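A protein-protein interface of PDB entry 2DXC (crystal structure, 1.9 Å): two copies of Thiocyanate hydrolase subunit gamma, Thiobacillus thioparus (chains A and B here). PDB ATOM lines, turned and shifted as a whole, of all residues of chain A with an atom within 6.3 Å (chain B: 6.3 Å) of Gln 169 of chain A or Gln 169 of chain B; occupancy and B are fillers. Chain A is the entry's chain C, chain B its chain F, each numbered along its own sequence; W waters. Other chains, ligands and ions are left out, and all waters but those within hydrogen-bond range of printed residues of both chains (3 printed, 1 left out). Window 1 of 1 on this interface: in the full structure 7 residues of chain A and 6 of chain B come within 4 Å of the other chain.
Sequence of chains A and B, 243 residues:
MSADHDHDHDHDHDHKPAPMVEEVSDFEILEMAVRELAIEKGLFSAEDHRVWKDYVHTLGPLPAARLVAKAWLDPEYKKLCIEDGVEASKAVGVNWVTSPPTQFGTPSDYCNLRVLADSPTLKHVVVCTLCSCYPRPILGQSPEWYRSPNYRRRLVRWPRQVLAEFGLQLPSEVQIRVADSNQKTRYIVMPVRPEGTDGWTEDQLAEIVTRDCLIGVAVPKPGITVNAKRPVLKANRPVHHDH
Gln 169 of chain B touches its own counterpart, Gln 169 of chain A.
Gln 169 of chain A touches Leu 170 of chain B, and with the chains exchanged Leu 170 of chain A touches Gln 169 of chain B.
Gln 169 of chain A touches Ser 172 of chain B, and with the chains exchanged Ser 172 of chain A touches Gln 169 of chain B.
Pro 171 of chain A touches Gln 169 of chain B, but with the chains exchanged Gln 169 of chain A does not touch Pro 171 of chain B (4.04 Å).
Of the 6 pairs that touch across the chains among the printed residues, 5 have their exchanged pair printed and touching as well.
O of Leu 170 of chain A lies within hydrogen-bond range of NH1 of Arg 160 of chain A (3.0 Å).
The guanidinium group (NH1) of Arg 160 of chain A lies within hydrogen-bond range of the backbone carbonyl oxygen (O) of Pro 171 of chain A (3.3 Å).
The guanidinium group (NH2) of Arg 160 of chain A lies within hydrogen-bond range of the backbone carbonyl oxygen (O) of Ser 172 of chain A, 3.4 Å away.
The guanidinium group (NH1) of Arg 160 of chain B sits at hydrogen-bond distance from the backbone carbonyl oxygen (O) of Leu 170 of chain B.
The backbone carbonyl oxygen (O) of Ser 172 of chain B lies within hydrogen-bond range of the guanidinium group (NH2) of Arg 160 of chain B (3.4 Å).
Along chain A the printed residues that touch a printed residue of chain B span positions 169 to 172.
Among the printed residues, 6 pairs touch across the chains.
Among the printed residues, no Asp or Glu carboxylate lies within 4 Å of a Lys or Arg side-chain nitrogen of the other chain.
Water W2 bridges the side-chain amide nitrogen of Gln 169 of chain A and the side-chain amide oxygen of Gln 169 of chain B.
Water W1 lies within hydrogen-bond range of NH1 of Arg 160 of chain A (2.9 Å), OE1 of Gln 169 of chain B (3.0 Å) and N of Leu 170 of chain A (3.0 Å).
Water W3 bridges the backbone carbonyl oxygen of Arg 160 of chain A (3.2 Å) and the backbone carbonyl oxygen of Arg 160 of chain B (3.4 Å).
OE1 of Gln 169 of chain A sits close to O of Leu 170 of chain B, at 2.9 Å.
The backbone carbonyl oxygen (O) of Leu 170 of chain A is in hydrogen-bond range of the side-chain amide nitrogen (NE2) of Gln 169 of chain B (2.7 Å).
Gln 169 of chain A touches just these residues of chain B: Gln 169 (3.4 Å), Leu 170 (2.9 Å) and Ser 172 (3.7 Å).
Of the printed residues of chain B, Leu 170 of chain A touches Gln 169.
Printed residues of chain B within 4 Å of Ser 172 of chain A: Gln 169 (3.7 Å).
Of the printed residues of chain A, Gln 169 of chain B touches Gln 169, Leu 170, Pro 171 and Ser 172.
Of the printed residues of chain A, Ser 172 of chain B touches Gln 169.
The nearest residue of chain B that does not touch Gln 169 of chain A is Pro 171 of chain B (4.04 Å).
Among the printed residues, pairs that only touch across the chains: Gln 169 of chain A with Gln 169 of chain B (3.4 Å), Gln 169 of chain A with Ser 172 of chain B (3.7 Å), Ser 172 of chain A with Gln 169 of chain B (3.7 Å) and Pro 171 of chain A with Gln 169 of chain B (3.98 Å).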
ATOM      1  N   ARG A 160       8.216 -15.499   0.432  1.00  0.00           N
ATOM      2  CA  ARG A 160       8.269 -15.229  -1.003  1.00  0.00           C
ATOM      3  C   ARG A 160       7.281 -14.121  -1.376  1.00  0.00           C
ATOM      4  O   ARG A 160       7.616 -13.198  -2.121  1.00  0.00           O
ATOM      5  CB  ARG A 160       7.947 -16.507  -1.794  1.00  0.00           C
ATOM      6  CG  ARG A 160       8.986 -17.633  -1.651  1.00  0.00           C
ATOM      7  CD  ARG A 160      10.198 -17.385  -2.532  1.00  0.00           C
ATOM      8  NE  ARG A 160      11.239 -18.404  -2.378  1.00  0.00           N
ATOM      9  CZ  ARG A 160      12.305 -18.496  -3.170  1.00  0.00           C
ATOM     10  NH1 ARG A 160      12.460 -17.635  -4.168  1.00  0.00           N
ATOM     11  NH2 ARG A 160      13.220 -19.435  -2.967  1.00  0.00           N
ATOM     12  N   LEU A 163       8.298 -10.603   0.496  1.00  0.00           N
ATOM     13  CA  LEU A 163       9.439  -9.976  -0.162  1.00  0.00           C
ATOM     14  C   LEU A 163       9.045  -9.403  -1.519  1.00  0.00           C
ATOM     15  O   LEU A 163       9.518  -8.336  -1.907  1.00  0.00           O
ATOM     16  CB  LEU A 163      10.583 -10.980  -0.324  1.00  0.00           C
ATOM     17  CG  LEU A 163      11.243 -11.407   0.986  1.00  0.00           C
ATOM     18  CD1 LEU A 163      12.350 -12.407   0.699  1.00  0.00           C
ATOM     19  CD2 LEU A 163      11.809 -10.180   1.698  1.00  0.00           C
ATOM     20  N   ALA A 164       8.177 -10.108  -2.239  1.00  0.00           N
ATOM     21  CA  ALA A 164       7.722  -9.631  -3.540  1.00  0.00           C
ATOM     22  C   ALA A 164       7.020  -8.286  -3.357  1.00  0.00           C
ATOM     23  O   ALA A 164       7.188  -7.371  -4.164  1.00  0.00           O
ATOM     24  CB  ALA A 164       6.770 -10.648  -4.174  1.00  0.00           C
ATOM     25  N   GLY A 167       9.252  -5.666  -3.365  1.00  0.00           N
ATOM     26  CA  GLY A 167       9.950  -5.499  -4.627  1.00  0.00           C
ATOM     27  C   GLY A 167      11.155  -6.413  -4.765  1.00  0.00           C
ATOM     28  O   GLY A 167      11.995  -6.213  -5.639  1.00  0.00           O
ATOM     29  N   LEU A 168      11.242  -7.429  -3.913  1.00  0.00           N
ATOM     30  CA  LEU A 168      12.366  -8.351  -3.960  1.00  0.00           C
ATOM     31  C   LEU A 168      11.966  -9.767  -4.346  1.00  0.00           C
ATOM     32  O   LEU A 168      11.093 -10.373  -3.725  1.00  0.00           O
ATOM     33  CB  LEU A 168      13.080  -8.379  -2.608  1.00  0.00           C
ATOM     34  CG  LEU A 168      14.242  -9.368  -2.490  1.00  0.00           C
ATOM     35  CD1 LEU A 168      15.272  -9.094  -3.589  1.00  0.00           C
ATOM     36  CD2 LEU A 168      14.875  -9.241  -1.116  1.00  0.00           C
ATOM     37  N   GLN A 169      12.625 -10.295  -5.369  1.00  0.00           N
ATOM     38  CA  GLN A 169      12.347 -11.642  -5.836  1.00  0.00           C
ATOM     39  C   GLN A 169      13.660 -12.372  -6.078  1.00  0.00           C
ATOM     40  O   GLN A 169      14.623 -11.779  -6.562  1.00  0.00           O
ATOM     41  CB  GLN A 169      11.533 -11.583  -7.129  1.00  0.00           C
ATOM     42  CG  GLN A 169      10.958 -12.914  -7.574  1.00  0.00           C
ATOM     43  CD  GLN A 169      10.039 -12.775  -8.780  1.00  0.00           C
ATOM     44  OE1 GLN A 169      10.473 -12.386  -9.867  1.00  0.00           O
ATOM     45  NE2 GLN A 169       8.761 -13.089  -8.591  1.00  0.00           N
ATOM     46  N   LEU A 170      13.704 -13.652  -5.727  1.00  0.00           N
ATOM     47  CA  LEU A 170      14.907 -14.443  -5.937  1.00  0.00           C
ATOM     48  C   LEU A 170      14.583 -15.740  -6.660  1.00  0.00           C
ATOM     49  O   LEU A 170      13.440 -16.201  -6.639  1.00  0.00           O
ATOM     50  CB  LEU A 170      15.596 -14.745  -4.604  1.00  0.00           C
ATOM     51  CG  LEU A 170      16.266 -13.520  -3.978  1.00  0.00           C
ATOM     52  CD1 LEU A 170      15.346 -12.898  -2.942  1.00  0.00           C
ATOM     53  CD2 LEU A 170      17.576 -13.932  -3.351  1.00  0.00           C
ATOM     54  N   PRO A 171      15.582 -16.337  -7.332  1.00  0.00           N
ATOM     55  CA  PRO A 171      15.360 -17.591  -8.054  1.00  0.00           C
ATOM     56  C   PRO A 171      14.690 -18.614  -7.143  1.00  0.00           C
ATOM     57  O   PRO A 171      14.981 -18.681  -5.949  1.00  0.00           O
ATOM     58  CB  PRO A 171      16.771 -18.007  -8.465  1.00  0.00           C
ATOM     59  CG  PRO A 171      17.452 -16.687  -8.676  1.00  0.00           C
ATOM     60  CD  PRO A 171      16.980 -15.888  -7.474  1.00  0.00           C
ATOM     61  N   SER A 172      13.790 -19.404  -7.711  1.00  0.00           N
ATOM     62  CA  SER A 172      13.074 -20.410  -6.943  1.00  0.00           C
ATOM     63  C   SER A 172      13.990 -21.433  -6.273  1.00  0.00           C
ATOM     64  O   SER A 172      13.650 -21.977  -5.220  1.00  0.00           O
ATOM     65  CB  SER A 172      12.064 -21.131  -7.840  1.00  0.00           C
ATOM     66  OG  SER A 172      12.717 -21.768  -8.923  1.00  0.00           O
ATOM     67  N   ARG B 160       1.599 -11.672  -8.617  1.00  0.00           N
ATOM     68  CA  ARG B 160       2.902 -12.279  -8.343  1.00  0.00           C
ATOM     69  C   ARG B 160       2.844 -13.156  -7.093  1.00  0.00           C
ATOM     70  O   ARG B 160       3.345 -14.283  -7.081  1.00  0.00           O
ATOM     71  CB  ARG B 160       3.953 -11.190  -8.128  1.00  0.00           C
ATOM     72  CG  ARG B 160       4.189 -10.280  -9.324  1.00  0.00           C
ATOM     73  CD  ARG B 160       5.235 -10.853 -10.243  1.00  0.00           C
ATOM     74  NE  ARG B 160       5.472 -10.018 -11.416  1.00  0.00           N
ATOM     75  CZ  ARG B 160       6.391 -10.290 -12.337  1.00  0.00           C
ATOM     76  NH1 ARG B 160       7.152 -11.367 -12.203  1.00  0.00           N
ATOM     77  NH2 ARG B 160       6.539  -9.502 -13.393  1.00  0.00           N
ATOM     78  N   LEU B 163       0.361 -16.312  -7.624  1.00  0.00           N
ATOM     79  CA  LEU B 163       0.972 -17.338  -8.473  1.00  0.00           C
ATOM     80  C   LEU B 163       2.093 -18.064  -7.724  1.00  0.00           C
ATOM     81  O   LEU B 163       2.270 -19.273  -7.880  1.00  0.00           O
ATOM     82  CB  LEU B 163       1.516 -16.722  -9.772  1.00  0.00           C
ATOM     83  CG  LEU B 163       0.485 -16.154 -10.763  1.00  0.00           C
ATOM     84  CD1 LEU B 163       1.192 -15.473 -11.924  1.00  0.00           C
ATOM     85  CD2 LEU B 163      -0.409 -17.278 -11.279  1.00  0.00           C
ATOM     86  N   ALA B 164       2.842 -17.328  -6.905  1.00  0.00           N
ATOM     87  CA  ALA B 164       3.929 -17.925  -6.133  1.00  0.00           C
ATOM     88  C   ALA B 164       3.348 -18.994  -5.213  1.00  0.00           C
ATOM     89  O   ALA B 164       3.948 -20.054  -5.018  1.00  0.00           O
ATOM     90  CB  ALA B 164       4.649 -16.856  -5.316  1.00  0.00           C
ATOM     91  N   GLY B 167       2.970 -21.929  -6.898  1.00  0.00           N
ATOM     92  CA  GLY B 167       4.245 -22.511  -7.286  1.00  0.00           C
ATOM     93  C   GLY B 167       4.812 -21.980  -8.593  1.00  0.00           C
ATOM     94  O   GLY B 167       5.737 -22.563  -9.161  1.00  0.00           O
ATOM     95  N   LEU B 168       4.266 -20.868  -9.071  1.00  0.00           N
ATOM     96  CA  LEU B 168       4.720 -20.272 -10.321  1.00  0.00           C
ATOM     97  C   LEU B 168       5.365 -18.911 -10.103  1.00  0.00           C
ATOM     98  O   LEU B 168       4.811 -18.048  -9.422  1.00  0.00           O
ATOM     99  CB  LEU B 168       3.541 -20.126 -11.287  1.00  0.00           C
ATOM    100  CG  LEU B 168       3.811 -19.425 -12.622  1.00  0.00           C
ATOM    101  CD1 LEU B 168       4.886 -20.176 -13.392  1.00  0.00           C
ATOM    102  CD2 LEU B 168       2.520 -19.361 -13.430  1.00  0.00           C
ATOM    103  N   GLN B 169       6.542 -18.724 -10.691  1.00  0.00           N
ATOM    104  CA  GLN B 169       7.261 -17.462 -10.578  1.00  0.00           C
ATOM    105  C   GLN B 169       7.906 -17.114 -11.916  1.00  0.00           C
ATOM    106  O   GLN B 169       8.470 -17.979 -12.583  1.00  0.00           O
ATOM    107  CB  GLN B 169       8.328 -17.560  -9.487  1.00  0.00           C
ATOM    108  CG  GLN B 169       9.252 -16.359  -9.411  1.00  0.00           C
ATOM    109  CD  GLN B 169      10.183 -16.421  -8.211  1.00  0.00           C
ATOM    110  OE1 GLN B 169       9.759 -16.227  -7.067  1.00  0.00           O
ATOM    111  NE2 GLN B 169      11.454 -16.701  -8.465  1.00  0.00           N
ATOM    112  N   LEU B 170       7.807 -15.846 -12.304  1.00  0.00           N
ATOM    113  CA  LEU B 170       8.382 -15.378 -13.558  1.00  0.00           C
ATOM    114  C   LEU B 170       9.356 -14.236 -13.313  1.00  0.00           C
ATOM    115  O   LEU B 170       9.293 -13.575 -12.277  1.00  0.00           O
ATOM    116  CB  LEU B 170       7.270 -14.920 -14.501  1.00  0.00           C
ATOM    117  CG  LEU B 170       6.492 -16.104 -15.078  1.00  0.00           C
ATOM    118  CD1 LEU B 170       5.020 -15.822 -15.066  1.00  0.00           C
ATOM    119  CD2 LEU B 170       7.003 -16.404 -16.475  1.00  0.00           C
ATOM    120  N   PRO B 171      10.275 -13.993 -14.263  1.00  0.00           N
ATOM    121  CA  PRO B 171      11.253 -12.911 -14.114  1.00  0.00           C
ATOM    122  C   PRO B 171      10.541 -11.592 -13.831  1.00  0.00           C
ATOM    123  O   PRO B 171       9.436 -11.361 -14.322  1.00  0.00           O
ATOM    124  CB  PRO B 171      11.969 -12.904 -15.462  1.00  0.00           C
ATOM    125  CG  PRO B 171      11.892 -14.351 -15.889  1.00  0.00           C
ATOM    126  CD  PRO B 171      10.469 -14.710 -15.537  1.00  0.00           C
ATOM    127  N   SER B 172      11.173 -10.729 -13.044  1.00  0.00           N
ATOM    128  CA  SER B 172      10.570  -9.449 -12.699  1.00  0.00           C
ATOM    129  C   SER B 172      10.320  -8.539 -13.902  1.00  0.00           C
ATOM    130  O   SER B 172       9.385  -7.740 -13.883  1.00  0.00           O
ATOM    131  CB  SER B 172      11.433  -8.725 -11.657  1.00  0.00           C
ATOM    132  OG  SER B 172      12.738  -8.483 -12.147  1.00  0.00           O
HETATM  133  O   HOH W   1      11.177 -15.053  -4.757  1.00  0.00           O
HETATM  134  O   HOH W   2       7.544 -14.157  -6.357  1.00  0.00           O
HETATM  135  O   HOH W   3       5.500 -13.688  -4.515  1.00  0.00           O
